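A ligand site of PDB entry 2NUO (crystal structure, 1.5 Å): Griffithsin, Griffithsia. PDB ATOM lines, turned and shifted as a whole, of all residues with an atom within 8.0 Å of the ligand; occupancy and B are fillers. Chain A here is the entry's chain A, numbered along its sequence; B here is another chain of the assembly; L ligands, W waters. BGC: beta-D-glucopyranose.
Merely in contact with the ligand: Gly 12 of chain B and Tyr 69. Hydrophobic or aromatic side chains within 4 Å of the ligand: Tyr 69 and Tyr 111.
The side-chain carboxylate (OD1) of Asp 113 lies within hydrogen-bond range of the backbone NH (N) of Gly 109, at 3.3 Å. The backbone carbonyl oxygen (O) of Ser 107 is in hydrogen-bond range of the backbone NH (N) of Asp 113, at 3.0 Å. The backbone carbonyl oxygen (O) of Asp 113 is in hydrogen-bond range of the backbone NH (N) of Gly 10 of chain B. N of Gly 42 lies within hydrogen-bond range of O of Asp 110, 3.2 Å away.
OD2 of Asp 113 sits at hydrogen-bond distance from O4 of the ligand (2.6 Å). The backbone NH of Tyr 111 is in hydrogen-bond range of an oxygen (O6) of the ligand (2.8 Å). The backbone carbonyl oxygen (O) of Tyr 111 lies within hydrogen-bond range of an oxygen (O6) of the ligand, 3.1 Å away. N of Asp 110 lies within hydrogen-bond range of O5 of the ligand. OD2 of Asp 110 lies within hydrogen-bond range of O1 of the ligand, 3.2 Å away. N of Gly 13 of chain B lies within hydrogen-bond range of O3 of the ligand (3.0 Å). The backbone NH (N) of Gly 109 sits at hydrogen-bond distance from an oxygen (O6) of the ligand.
Water W4 bridges OH of Tyr 69 (2.8 Å) and O4 of the ligand (3.1 Å). Water W1 bridges OG of Ser 14 of chain B (3.1 Å) and O3 of the ligand (3.3 Å).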
ATOM      1  N   TYR A  29       2.353 -27.791  18.892  1.00  0.00           N
ATOM      2  CA  TYR A  29       3.362 -28.843  18.679  1.00  0.00           C
ATOM      3  C   TYR A  29       4.060 -29.126  19.992  1.00  0.00           C
ATOM      4  O   TYR A  29       3.756 -28.548  21.056  1.00  0.00           O
ATOM      5  CB  TYR A  29       4.465 -28.418  17.700  1.00  0.00           C
ATOM      6  CG  TYR A  29       3.990 -27.852  16.395  1.00  0.00           C
ATOM      7  CD1 TYR A  29       2.913 -28.387  15.729  1.00  0.00           C
ATOM      8  CD2 TYR A  29       4.692 -26.801  15.800  1.00  0.00           C
ATOM      9  CE1 TYR A  29       2.515 -27.866  14.468  1.00  0.00           C
ATOM     10  CE2 TYR A  29       4.290 -26.263  14.589  1.00  0.00           C
ATOM     11  CZ  TYR A  29       3.201 -26.815  13.901  1.00  0.00           C
ATOM     12  OH  TYR A  29       2.724 -26.309  12.659  1.00  0.00           O
ATOM     13  N   LEU A  30       4.972 -30.075  19.944  1.00  0.00           N
ATOM     14  CA  LEU A  30       5.932 -30.185  21.026  1.00  0.00           C
ATOM     15  C   LEU A  30       7.109 -29.265  20.702  1.00  0.00           C
ATOM     16  O   LEU A  30       7.873 -29.549  19.793  1.00  0.00           O
ATOM     17  CB  LEU A  30       6.446 -31.619  21.210  1.00  0.00           C
ATOM     18  CG  LEU A  30       5.444 -32.643  21.779  1.00  0.00           C
ATOM     19  CD1 LEU A  30       6.128 -33.912  22.269  1.00  0.00           C
ATOM     20  CD2 LEU A  30       4.506 -32.121  22.893  1.00  0.00           C
ATOM     21  N   ASP A  31       7.227 -28.209  21.467  1.00  0.00           N
ATOM     22  CA  ASP A  31       8.340 -27.274  21.372  1.00  0.00           C
ATOM     23  C   ASP A  31       9.623 -27.905  21.872  1.00  0.00           C
ATOM     24  O   ASP A  31      10.704 -27.619  21.364  1.00  0.00           O
ATOM     25  CB  ASP A  31       8.012 -26.028  22.137  1.00  0.00           C
ATOM     26  CG  ASP A  31       6.823 -25.244  21.514  1.00  0.00           C
ATOM     27  OD1 ASP A  31       5.649 -25.602  21.772  1.00  0.00           O
ATOM     28  OD2 ASP A  31       7.091 -24.306  20.695  1.00  0.00           O
ATOM     29  N   GLY A  41      15.019 -28.744  22.467  1.00  0.00           N
ATOM     30  CA  GLY A  41      14.072 -27.983  21.677  1.00  0.00           C
ATOM     31  C   GLY A  41      14.060 -26.509  22.012  1.00  0.00           C
ATOM     32  O   GLY A  41      15.106 -25.992  22.414  1.00  0.00           O
ATOM     33  N   GLY A  42      12.990 -25.811  21.698  1.00  0.00           N
ATOM     34  CA  GLY A  42      12.883 -24.381  21.819  1.00  0.00           C
ATOM     35  C   GLY A  42      12.191 -23.906  23.066  1.00  0.00           C
ATOM     36  O   GLY A  42      11.939 -24.653  24.021  1.00  0.00           O
ATOM     37  N   ASP A  68       5.722 -32.884  10.067  1.00  0.00           N
ATOM     38  CA  ASP A  68       7.106 -32.333   9.930  1.00  0.00           C
ATOM     39  C   ASP A  68       7.780 -32.307  11.316  1.00  0.00           C
ATOM     40  O   ASP A  68       8.998 -32.480  11.421  1.00  0.00           O
ATOM     41  CB  ASP A  68       7.122 -30.920   9.367  1.00  0.00           C
ATOM     42  CG  ASP A  68       6.774 -30.844   7.897  1.00  0.00           C
ATOM     43  OD1 ASP A  68       7.030 -31.807   7.160  1.00  0.00           O
ATOM     44  OD2 ASP A  68       6.266 -29.771   7.516  1.00  0.00           O
ATOM     45  N   TYR A  69       6.963 -32.143  12.366  1.00  0.00           N
ATOM     46  CA  TYR A  69       7.408 -32.094  13.767  1.00  0.00           C
ATOM     47  C   TYR A  69       6.661 -33.106  14.612  1.00  0.00           C
ATOM     48  O   TYR A  69       5.801 -33.843  14.117  1.00  0.00           O
ATOM     49  CB  TYR A  69       7.190 -30.683  14.377  1.00  0.00           C
ATOM     50  CG  TYR A  69       7.634 -29.566  13.448  1.00  0.00           C
ATOM     51  CD1 TYR A  69       8.924 -29.514  12.996  1.00  0.00           C
ATOM     52  CD2 TYR A  69       6.767 -28.558  13.093  1.00  0.00           C
ATOM     53  CE1 TYR A  69       9.376 -28.541  12.126  1.00  0.00           C
ATOM     54  CE2 TYR A  69       7.176 -27.540  12.192  1.00  0.00           C
ATOM     55  CZ  TYR A  69       8.482 -27.577  11.718  1.00  0.00           C
ATOM     56  OH  TYR A  69       8.874 -26.595  10.845  1.00  0.00           O
ATOM     57  N   SER A 107      15.565 -35.540  17.474  1.00  0.00           N
ATOM     58  CA  SER A 107      16.186 -34.389  16.839  1.00  0.00           C
ATOM     59  C   SER A 107      15.345 -33.162  17.152  1.00  0.00           C
ATOM     60  O   SER A 107      14.098 -33.217  17.129  1.00  0.00           O
ATOM     61  CB  SER A 107      16.336 -34.530  15.341  1.00  0.00           C
ATOM     62  OG  SER A 107      17.295 -35.545  15.030  1.00  0.00           O
ATOM     63  N   ALA A 108      16.004 -32.026  17.375  1.00  0.00           N
ATOM     64  CA  ALA A 108      15.307 -30.807  17.758  1.00  0.00           C
ATOM     65  C   ALA A 108      15.981 -29.557  17.246  1.00  0.00           C
ATOM     66  O   ALA A 108      17.203 -29.549  17.094  1.00  0.00           O
ATOM     67  CB  ALA A 108      15.179 -30.734  19.274  1.00  0.00           C
ATOM     68  N   GLY A 109      15.195 -28.532  17.073  1.00  0.00           N
ATOM     69  CA  GLY A 109      15.672 -27.178  16.754  1.00  0.00           C
ATOM     70  C   GLY A 109      14.865 -26.206  17.620  1.00  0.00           C
ATOM     71  O   GLY A 109      15.023 -26.180  18.848  1.00  0.00           O
ATOM     72  N   ASP A 110      14.035 -25.408  16.953  1.00  0.00           N
ATOM     73  CA  ASP A 110      13.065 -24.555  17.647  1.00  0.00           C
ATOM     74  C   ASP A 110      11.893 -25.425  18.180  1.00  0.00           C
ATOM     75  O   ASP A 110      11.208 -25.036  19.111  1.00  0.00           O
ATOM     76  CB  ASP A 110      12.501 -23.498  16.712  1.00  0.00           C
ATOM     77  CG  ASP A 110      13.573 -22.501  16.246  1.00  0.00           C
ATOM     78  OD1 ASP A 110      14.476 -22.157  17.049  1.00  0.00           O
ATOM     79  OD2 ASP A 110      13.541 -22.031  15.077  1.00  0.00           O
ATOM     80  N   TYR A 111      11.673 -26.576  17.552  1.00  0.00           N
ATOM     81  CA  TYR A 111      10.686 -27.551  17.978  1.00  0.00           C
ATOM     82  C   TYR A 111      11.300 -28.899  18.129  1.00  0.00           C
ATOM     83  O   TYR A 111      12.461 -29.111  17.810  1.00  0.00           O
ATOM     84  CB  TYR A 111       9.528 -27.679  16.972  1.00  0.00           C
ATOM     85  CG  TYR A 111       8.808 -26.382  16.572  1.00  0.00           C
ATOM     86  CD1 TYR A 111       8.307 -25.517  17.513  1.00  0.00           C
ATOM     87  CD2 TYR A 111       8.549 -26.144  15.242  1.00  0.00           C
ATOM     88  CE1 TYR A 111       7.630 -24.364  17.163  1.00  0.00           C
ATOM     89  CE2 TYR A 111       7.921 -24.992  14.857  1.00  0.00           C
ATOM     90  CZ  TYR A 111       7.411 -24.132  15.807  1.00  0.00           C
ATOM     91  OH  TYR A 111       6.738 -23.010  15.368  1.00  0.00           O
ATOM     92  N   LEU A 112      10.521 -29.843  18.638  1.00  0.00           N
ATOM     93  CA  LEU A 112      10.912 -31.225  18.589  1.00  0.00           C
ATOM     94  C   LEU A 112      10.580 -31.775  17.212  1.00  0.00           C
ATOM     95  O   LEU A 112       9.408 -31.992  16.923  1.00  0.00           O
ATOM     96  CB  LEU A 112      10.155 -31.999  19.691  1.00  0.00           C
ATOM     97  CG  LEU A 112      10.518 -33.431  19.827  1.00  0.00           C
ATOM     98  CD1 LEU A 112      12.027 -33.672  20.168  1.00  0.00           C
ATOM     99  CD2 LEU A 112       9.644 -34.028  20.904  1.00  0.00           C
ATOM    100  N   ASP A 113      11.568 -31.928  16.326  1.00  0.00           N
ATOM    101  CA  ASP A 113      11.348 -32.413  14.983  1.00  0.00           C
ATOM    102  C   ASP A 113      10.983 -33.885  14.936  1.00  0.00           C
ATOM    103  O   ASP A 113      10.180 -34.305  14.106  1.00  0.00           O
ATOM    104  CB  ASP A 113      12.576 -32.221  14.126  1.00  0.00           C
ATOM    105  CG  ASP A 113      12.870 -30.776  13.897  1.00  0.00           C
ATOM    106  OD1 ASP A 113      13.410 -30.140  14.802  1.00  0.00           O
ATOM    107  OD2 ASP A 113      12.448 -30.220  12.850  1.00  0.00           O
ATOM    108  N   SER A 114      11.670 -34.685  15.737  1.00  0.00           N
ATOM    109  CA  SER A 114      11.542 -36.098  15.697  1.00  0.00           C
ATOM    110  C   SER A 114      11.978 -36.798  16.996  1.00  0.00           C
ATOM    111  O   SER A 114      12.686 -36.229  17.798  1.00  0.00           O
ATOM    112  CB  SER A 114      12.314 -36.720  14.550  1.00  0.00           C
ATOM    113  OG  SER A 114      13.696 -36.552  14.668  1.00  0.00           O
ATOM    114  N   GLY B  10       9.694 -35.541  11.441  1.00  0.00           N
ATOM    115  CA  GLY B  10      10.296 -35.103  10.206  1.00  0.00           C
ATOM    116  C   GLY B  10      11.804 -35.161  10.165  1.00  0.00           C
ATOM    117  O   GLY B  10      12.434 -35.778  11.009  1.00  0.00           O
ATOM    118  N   SER B  11      12.381 -34.512   9.156  1.00  0.00           N
ATOM    119  CA  SER B  11      13.803 -34.685   8.848  1.00  0.00           C
ATOM    120  C   SER B  11      14.681 -33.607   9.478  1.00  0.00           C
ATOM    121  O   SER B  11      15.923 -33.727   9.408  1.00  0.00           O
ATOM    122  CB  SER B  11      13.989 -34.653   7.299  1.00  0.00           C
ATOM    123  OG  SER B  11      13.535 -33.421   6.800  1.00  0.00           O
ATOM    124  N   GLY B  12      14.117 -32.575  10.095  1.00  0.00           N
ATOM    125  CA  GLY B  12      14.867 -31.415  10.559  1.00  0.00           C
ATOM    126  C   GLY B  12      15.467 -31.597  11.948  1.00  0.00           C
ATOM    127  O   GLY B  12      15.378 -32.677  12.556  1.00  0.00           O
ATOM    128  N   GLY B  13      16.084 -30.537  12.458  1.00  0.00           N
ATOM    129  CA  GLY B  13      16.635 -30.533  13.769  1.00  0.00           C
ATOM    130  C   GLY B  13      17.978 -31.191  13.853  1.00  0.00           C
ATOM    131  O   GLY B  13      18.423 -31.812  12.959  1.00  0.00           O
ATOM    132  N   SER B  14      18.529 -31.113  15.052  1.00  0.00           N
ATOM    133  CA  SER B  14      19.823 -31.680  15.390  1.00  0.00           C
ATOM    134  C   SER B  14      19.661 -32.810  16.411  1.00  0.00           C
ATOM    135  O   SER B  14      18.939 -32.669  17.416  1.00  0.00           O
ATOM    136  CB  SER B  14      20.765 -30.614  15.992  1.00  0.00           C
ATOM    137  OG  SER B  14      21.008 -29.622  15.012  1.00  0.00           O
HETATM  138  C2  BGC L   1      16.240 -25.858  12.708  1.00  0.00           C
HETATM  139  C3  BGC L   1      15.561 -26.803  11.767  1.00  0.00           C
HETATM  140  C4  BGC L   1      14.357 -27.456  12.477  1.00  0.00           C
HETATM  141  C5  BGC L   1      13.536 -26.377  13.136  1.00  0.00           C
HETATM  142  C6  BGC L   1      12.331 -26.877  13.964  1.00  0.00           C
HETATM  143  C1  BGC L   1      15.244 -24.825  13.190  1.00  0.00           C
HETATM  144  O1  BGC L   1      15.869 -23.915  14.042  1.00  0.00           O
HETATM  145  O2  BGC L   1      17.362 -25.202  12.089  1.00  0.00           O
HETATM  146  O3  BGC L   1      16.365 -27.778  11.237  1.00  0.00           O
HETATM  147  O4  BGC L   1      13.540 -28.219  11.615  1.00  0.00           O
HETATM  148  O5  BGC L   1      14.216 -25.447  13.969  1.00  0.00           O
HETATM  149  O6  BGC L   1      12.834 -27.518  15.158  1.00  0.00           O
HETATM  150  O   HOH W   1      18.904 -27.930  13.409  1.00  0.00           O
HETATM  151  O   HOH W   2      19.115 -25.601  14.770  1.00  0.00           O
HETATM  152  O   HOH W   3      17.449 -24.373  16.528  1.00  0.00           O
HETATM  153  O   HOH W   4      11.504 -26.491  10.038  1.00  0.00           O
